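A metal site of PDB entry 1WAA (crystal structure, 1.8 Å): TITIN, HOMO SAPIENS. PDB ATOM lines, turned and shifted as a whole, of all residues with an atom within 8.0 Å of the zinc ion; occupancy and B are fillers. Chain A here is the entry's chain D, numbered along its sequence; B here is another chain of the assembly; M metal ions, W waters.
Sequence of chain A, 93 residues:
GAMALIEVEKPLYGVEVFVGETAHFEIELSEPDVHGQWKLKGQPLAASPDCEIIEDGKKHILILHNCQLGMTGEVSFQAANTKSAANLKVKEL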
ATOM      1  N   THR A  22     -22.417   2.619 -30.332  1.00  0.00           N
ATOM      2  CA  THR A  22     -22.225   3.200 -28.996  1.00  0.00           C
ATOM      3  C   THR A  22     -20.743   3.532 -28.772  1.00  0.00           C
ATOM      4  O   THR A  22     -19.839   2.852 -29.295  1.00  0.00           O
ATOM      5  CB  THR A  22     -22.810   2.307 -27.833  1.00  0.00           C
ATOM      6  OG1 THR A  22     -21.777   1.784 -26.981  1.00  0.00           O
ATOM      7  CG2 THR A  22     -23.610   1.129 -28.320  1.00  0.00           C
ATOM      8  N   SER A  48     -29.816   7.816 -18.360  1.00  0.00           N
ATOM      9  CA  SER A  48     -30.989   7.349 -19.119  1.00  0.00           C
ATOM     10  C   SER A  48     -30.556   6.074 -19.808  1.00  0.00           C
ATOM     11  O   SER A  48     -29.357   5.727 -19.779  1.00  0.00           O
ATOM     12  CB  SER A  48     -31.474   8.376 -20.163  1.00  0.00           C
ATOM     13  OG  SER A  48     -30.497   8.562 -21.173  1.00  0.00           O
ATOM     14  N   PRO A  49     -31.452   5.296 -20.426  1.00  0.00           N
ATOM     15  CA  PRO A  49     -31.045   4.096 -21.134  1.00  0.00           C
ATOM     16  C   PRO A  49     -29.947   4.289 -22.172  1.00  0.00           C
ATOM     17  O   PRO A  49     -29.183   3.327 -22.403  1.00  0.00           O
ATOM     18  CB  PRO A  49     -32.343   3.553 -21.699  1.00  0.00           C
ATOM     19  CG  PRO A  49     -33.468   4.389 -21.176  1.00  0.00           C
ATOM     20  CD  PRO A  49     -32.905   5.564 -20.449  1.00  0.00           C
ATOM     21  N   ASP A  50     -29.844   5.465 -22.750  1.00  0.00           N
ATOM     22  CA  ASP A  50     -28.841   5.718 -23.810  1.00  0.00           C
ATOM     23  C   ASP A  50     -27.642   6.544 -23.349  1.00  0.00           C
ATOM     24  O   ASP A  50     -26.750   6.853 -24.148  1.00  0.00           O
ATOM     25  CB  ASP A  50     -29.488   6.482 -24.965  1.00  0.00           C
ATOM     26  CG  ASP A  50     -30.343   5.592 -25.824  1.00  0.00           C
ATOM     27  OD1 ASP A  50     -30.228   4.330 -25.729  1.00  0.00           O
ATOM     28  OD2 ASP A  50     -31.173   6.107 -26.635  1.00  0.00           O
ATOM     29  N   CYS A  51     -27.641   6.896 -22.101  1.00  0.00           N
ATOM     30  CA  CYS A  51     -26.578   7.678 -21.512  1.00  0.00           C
ATOM     31  C   CYS A  51     -26.377   7.102 -20.138  1.00  0.00           C
ATOM     32  O   CYS A  51     -27.032   7.495 -19.184  1.00  0.00           O
ATOM     33  CB  CYS A  51     -27.017   9.144 -21.436  1.00  0.00           C
ATOM     34  SG  CYS A  51     -25.721  10.235 -20.744  1.00  0.00           S
ATOM     35  N   GLU A  52     -25.473   6.132 -20.045  1.00  0.00           N
ATOM     36  CA  GLU A  52     -25.243   5.461 -18.753  1.00  0.00           C
ATOM     37  C   GLU A  52     -23.951   5.979 -18.105  1.00  0.00           C
ATOM     38  O   GLU A  52     -22.897   6.005 -18.715  1.00  0.00           O
ATOM     39  CB  GLU A  52     -25.209   3.946 -19.008  1.00  0.00           C
ATOM     40  CG  GLU A  52     -26.601   3.449 -19.452  1.00  0.00           C
ATOM     41  CD  GLU A  52     -26.619   2.100 -20.134  1.00  0.00           C
ATOM     42  OE1 GLU A  52     -27.570   1.288 -19.883  1.00  0.00           O
ATOM     43  OE2 GLU A  52     -25.702   1.784 -20.958  1.00  0.00           O
ATOM     44  N   ILE A  54     -21.442   5.523 -15.028  1.00  0.00           N
ATOM     45  CA  ILE A  54     -20.957   4.441 -14.175  1.00  0.00           C
ATOM     46  C   ILE A  54     -19.765   4.855 -13.288  1.00  0.00           C
ATOM     47  O   ILE A  54     -18.863   5.565 -13.716  1.00  0.00           O
ATOM     48  CB  ILE A  54     -20.499   3.305 -15.121  1.00  0.00           C
ATOM     49  CG1 ILE A  54     -21.645   2.825 -16.068  1.00  0.00           C
ATOM     50  CG2 ILE A  54     -19.962   2.080 -14.374  1.00  0.00           C
ATOM     51  CD1 ILE A  54     -22.773   2.068 -15.365  1.00  0.00           C
ATOM     52  N   ILE A  63     -21.268   5.649 -21.020  1.00  0.00           N
ATOM     53  CA  ILE A  63     -21.660   4.865 -22.202  1.00  0.00           C
ATOM     54  C   ILE A  63     -22.766   5.626 -22.906  1.00  0.00           C
ATOM     55  O   ILE A  63     -23.798   5.926 -22.317  1.00  0.00           O
ATOM     56  CB  ILE A  63     -22.154   3.473 -21.822  1.00  0.00           C
ATOM     57  CG1 ILE A  63     -21.043   2.657 -21.155  1.00  0.00           C
ATOM     58  CG2 ILE A  63     -22.660   2.665 -23.045  1.00  0.00           C
ATOM     59  CD1 ILE A  63     -21.531   1.384 -20.515  1.00  0.00           C
ATOM     60  N   LEU A  64     -22.517   5.929 -24.157  1.00  0.00           N
ATOM     61  CA  LEU A  64     -23.491   6.649 -24.966  1.00  0.00           C
ATOM     62  C   LEU A  64     -23.950   5.730 -26.093  1.00  0.00           C
ATOM     63  O   LEU A  64     -23.185   5.433 -27.019  1.00  0.00           O
ATOM     64  CB  LEU A  64     -22.865   7.912 -25.568  1.00  0.00           C
ATOM     65  CG  LEU A  64     -22.406   8.945 -24.559  1.00  0.00           C
ATOM     66  CD1 LEU A  64     -21.490   9.993 -25.236  1.00  0.00           C
ATOM     67  CD2 LEU A  64     -23.584   9.659 -23.907  1.00  0.00           C
ATOM     68  N   HIS A  65     -25.195   5.284 -26.010  1.00  0.00           N
ATOM     69  CA  HIS A  65     -25.770   4.391 -27.028  1.00  0.00           C
ATOM     70  C   HIS A  65     -26.435   5.184 -28.147  1.00  0.00           C
ATOM     71  O   HIS A  65     -26.877   6.311 -27.942  1.00  0.00           O
ATOM     72  CB  HIS A  65     -26.857   3.509 -26.413  1.00  0.00           C
ATOM     73  CG  HIS A  65     -26.326   2.479 -25.441  1.00  0.00           C
ATOM     74  ND1 HIS A  65     -25.388   1.529 -25.822  1.00  0.00           N
ATOM     75  CD2 HIS A  65     -26.613   2.254 -24.140  1.00  0.00           C
ATOM     76  CE1 HIS A  65     -25.129   0.776 -24.765  1.00  0.00           C
ATOM     77  NE2 HIS A  65     -25.857   1.192 -23.755  1.00  0.00           N
ATOM     78  N   LYS B  10     -31.018  -6.912 -19.782  1.00  0.00           N
ATOM     79  CA  LYS B  10     -30.436  -6.549 -21.083  1.00  0.00           C
ATOM     80  C   LYS B  10     -29.204  -7.416 -21.288  1.00  0.00           C
ATOM     81  O   LYS B  10     -28.242  -7.311 -20.522  1.00  0.00           O
ATOM     82  CB  LYS B  10     -30.055  -5.058 -21.101  1.00  0.00           C
ATOM     83  CG  LYS B  10     -31.168  -4.123 -20.673  1.00  0.00           C
ATOM     84  N   TYR B  13     -24.321  -8.259 -25.785  1.00  0.00           N
ATOM     85  CA  TYR B  13     -24.430  -8.204 -27.238  1.00  0.00           C
ATOM     86  C   TYR B  13     -23.023  -8.363 -27.861  1.00  0.00           C
ATOM     87  O   TYR B  13     -22.032  -7.978 -27.246  1.00  0.00           O
ATOM     88  CB  TYR B  13     -25.172  -6.935 -27.721  1.00  0.00           C
ATOM     89  CG  TYR B  13     -24.638  -5.647 -27.128  1.00  0.00           C
ATOM     90  CD1 TYR B  13     -25.296  -5.017 -26.054  1.00  0.00           C
ATOM     91  CD2 TYR B  13     -23.461  -5.061 -27.619  1.00  0.00           C
ATOM     92  CE1 TYR B  13     -24.790  -3.816 -25.483  1.00  0.00           C
ATOM     93  CE2 TYR B  13     -22.937  -3.876 -27.054  1.00  0.00           C
ATOM     94  CZ  TYR B  13     -23.608  -3.262 -25.992  1.00  0.00           C
ATOM     95  OH  TYR B  13     -23.081  -2.101 -25.455  1.00  0.00           O
ATOM     96  N   HIS B  24     -15.883  -3.389 -25.394  1.00  0.00           N
ATOM     97  CA  HIS B  24     -16.611  -3.309 -24.153  1.00  0.00           C
ATOM     98  C   HIS B  24     -17.905  -4.128 -24.276  1.00  0.00           C
ATOM     99  O   HIS B  24     -18.615  -4.074 -25.275  1.00  0.00           O
ATOM    100  CB  HIS B  24     -16.759  -1.812 -23.705  1.00  0.00           C
ATOM    101  CG  HIS B  24     -18.156  -1.240 -23.773  1.00  0.00           C
ATOM    102  ND1 HIS B  24     -18.491  -0.189 -24.615  1.00  0.00           N
ATOM    103  CD2 HIS B  24     -19.281  -1.526 -23.062  1.00  0.00           C
ATOM    104  CE1 HIS B  24     -19.768   0.123 -24.443  1.00  0.00           C
ATOM    105  NE2 HIS B  24     -20.276  -0.686 -23.524  1.00  0.00           N
ATOM    106  N   PHE B  25     -18.153  -4.914 -23.225  1.00  0.00           N
ATOM    107  CA  PHE B  25     -19.372  -5.708 -23.089  1.00  0.00           C
ATOM    108  C   PHE B  25     -20.129  -5.216 -21.895  1.00  0.00           C
ATOM    109  O   PHE B  25     -19.521  -4.733 -20.922  1.00  0.00           O
ATOM    110  CB  PHE B  25     -19.022  -7.175 -22.907  1.00  0.00           C
ATOM    111  CG  PHE B  25     -18.482  -7.806 -24.168  1.00  0.00           C
ATOM    112  CD1 PHE B  25     -19.349  -8.455 -25.042  1.00  0.00           C
ATOM    113  CD2 PHE B  25     -17.129  -7.712 -24.478  1.00  0.00           C
ATOM    114  CE1 PHE B  25     -18.854  -9.030 -26.232  1.00  0.00           C
ATOM    115  CE2 PHE B  25     -16.617  -8.288 -25.645  1.00  0.00           C
ATOM    116  CZ  PHE B  25     -17.500  -8.944 -26.531  1.00  0.00           C
ATOM    117  N   GLU B  26     -21.441  -5.369 -21.932  1.00  0.00           N
ATOM    118  CA  GLU B  26     -22.270  -4.934 -20.820  1.00  0.00           C
ATOM    119  C   GLU B  26     -23.539  -5.750 -20.724  1.00  0.00           C
ATOM    120  O   GLU B  26     -24.108  -6.149 -21.734  1.00  0.00           O
ATOM    121  CB  GLU B  26     -22.604  -3.440 -20.908  1.00  0.00           C
ATOM    122  CG  GLU B  26     -23.332  -3.039 -22.173  1.00  0.00           C
ATOM    123  CD  GLU B  26     -23.758  -1.591 -22.195  1.00  0.00           C
ATOM    124  OE1 GLU B  26     -24.886  -1.288 -21.739  1.00  0.00           O
ATOM    125  OE2 GLU B  26     -22.984  -0.756 -22.717  1.00  0.00           O
ATOM    126  N   ILE B  27     -23.958  -5.976 -19.479  1.00  0.00           N
ATOM    127  CA  ILE B  27     -25.152  -6.710 -19.188  1.00  0.00           C
ATOM    128  C   ILE B  27     -25.868  -6.042 -17.984  1.00  0.00           C
ATOM    129  O   ILE B  27     -25.213  -5.516 -17.065  1.00  0.00           O
ATOM    130  CB  ILE B  27     -24.810  -8.223 -18.924  1.00  0.00           C
ATOM    131  CG1 ILE B  27     -26.098  -9.029 -18.679  1.00  0.00           C
ATOM    132  CG2 ILE B  27     -23.853  -8.382 -17.748  1.00  0.00           C
ATOM    133  CD1 ILE B  27     -25.840 -10.582 -18.592  1.00  0.00           C
ATOM    134  N   GLU B  28     -27.199  -6.023 -18.043  1.00  0.00           N
ATOM    135  CA  GLU B  28     -27.985  -5.458 -16.960  1.00  0.00           C
ATOM    136  C   GLU B  28     -28.806  -6.572 -16.312  1.00  0.00           C
ATOM    137  O   GLU B  28     -29.528  -7.319 -16.999  1.00  0.00           O
ATOM    138  CB  GLU B  28     -28.921  -4.393 -17.503  1.00  0.00           C
ATOM    139  CG  GLU B  28     -29.521  -3.454 -16.433  1.00  0.00           C
ATOM    140  CD  GLU B  28     -30.421  -2.401 -17.090  1.00  0.00           C
ATOM    141  OE1 GLU B  28     -29.863  -1.552 -17.828  1.00  0.00           O
ATOM    142  OE2 GLU B  28     -31.679  -2.433 -16.897  1.00  0.00           O
ATOM    143  N   LYS B  59     -25.745  -3.034 -13.394  1.00  0.00           N
ATOM    144  CA  LYS B  59     -24.888  -3.082 -14.570  1.00  0.00           C
ATOM    145  C   LYS B  59     -23.563  -3.762 -14.296  1.00  0.00           C
ATOM    146  O   LYS B  59     -22.895  -3.470 -13.311  1.00  0.00           O
ATOM    147  CB  LYS B  59     -24.605  -1.665 -15.094  1.00  0.00           C
ATOM    148  CG  LYS B  59     -25.744  -1.065 -15.878  1.00  0.00           C
ATOM    149  CD  LYS B  59     -25.708  -1.527 -17.348  1.00  0.00           C
ATOM    150  CE  LYS B  59     -26.779  -0.781 -18.095  1.00  0.00           C
ATOM    151  NZ  LYS B  59     -27.582  -1.614 -18.998  1.00  0.00           N
ATOM    152  N   ILE B  61     -19.922  -4.577 -16.447  1.00  0.00           N
ATOM    153  CA  ILE B  61     -19.166  -4.181 -17.634  1.00  0.00           C
ATOM    154  C   ILE B  61     -17.806  -4.856 -17.690  1.00  0.00           C
ATOM    155  O   ILE B  61     -17.159  -5.046 -16.656  1.00  0.00           O
ATOM    156  CB  ILE B  61     -19.072  -2.635 -17.681  1.00  0.00           C
ATOM    157  CG1 ILE B  61     -20.438  -2.066 -18.039  1.00  0.00           C
ATOM    158  CG2 ILE B  61     -18.024  -2.138 -18.714  1.00  0.00           C
ATOM    159  CD1 ILE B  61     -20.710  -0.722 -17.424  1.00  0.00           C
HETATM  160 ZN    ZN M   1     -25.831   0.208 -22.049  1.00  0.00          ZN
HETATM  161  O   HOH W   1     -27.681  -0.680 -21.890  1.00  0.00           O
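The zinc ion is bound by the side-chain carboxylate (OE1) of Glu 26 of chain B (1.8 Å), the side-chain carboxylate (OE2) of Glu 52 (1.9 Å), a ring nitrogen (NE2) of His 65 (2.0 Å) and water W1 (2.1 Å).
The zinc ion has four donor atoms within binding distance.
Merely in contact with the zinc ion: Lys 59 of chain B (3.96 Å).
Four residues have an atom within 4 Å of the zinc ion: Glu 52, His 65, Glu 26 of chain B and Lys 59 of chain B.
The nearest printed residue that does not touch the zinc ion is Ile 63 (4.1 Å).
The side-chain carboxylate (OE1) of Glu 26 of chain B sits close to the side-chain amino group (NZ) of Lys 59 of chain B, 3.9 Å away.
The side-chain carboxylate of Glu 26 of chain B sits at hydrogen-bond distance from the side-chain hydroxyl of Tyr 13 of chain B (3.1 Å).
OE2 of Glu 26 of chain B lies within hydrogen-bond range of NE2 of His 24 of chain B, at 2.8 Å.
OE1 of Glu 52 lies within salt-bridge range of NZ of Lys 59 of chain B (3.0 Å).
N of Glu 52 is in hydrogen-bond range of O of Ile 63, at 2.8 Å.
N of His 65 is in hydrogen-bond range of O of Asp 50 (2.9 Å).
The side-chain amino group of Lys 59 of chain B is in salt-bridge range of the side-chain carboxylate of Glu 28 of chain B (2.6 Å).
Water W1 bridges OE1 of Glu 52 (2.8 Å) and NZ of Lys 59 of chain B (3.0 Å).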
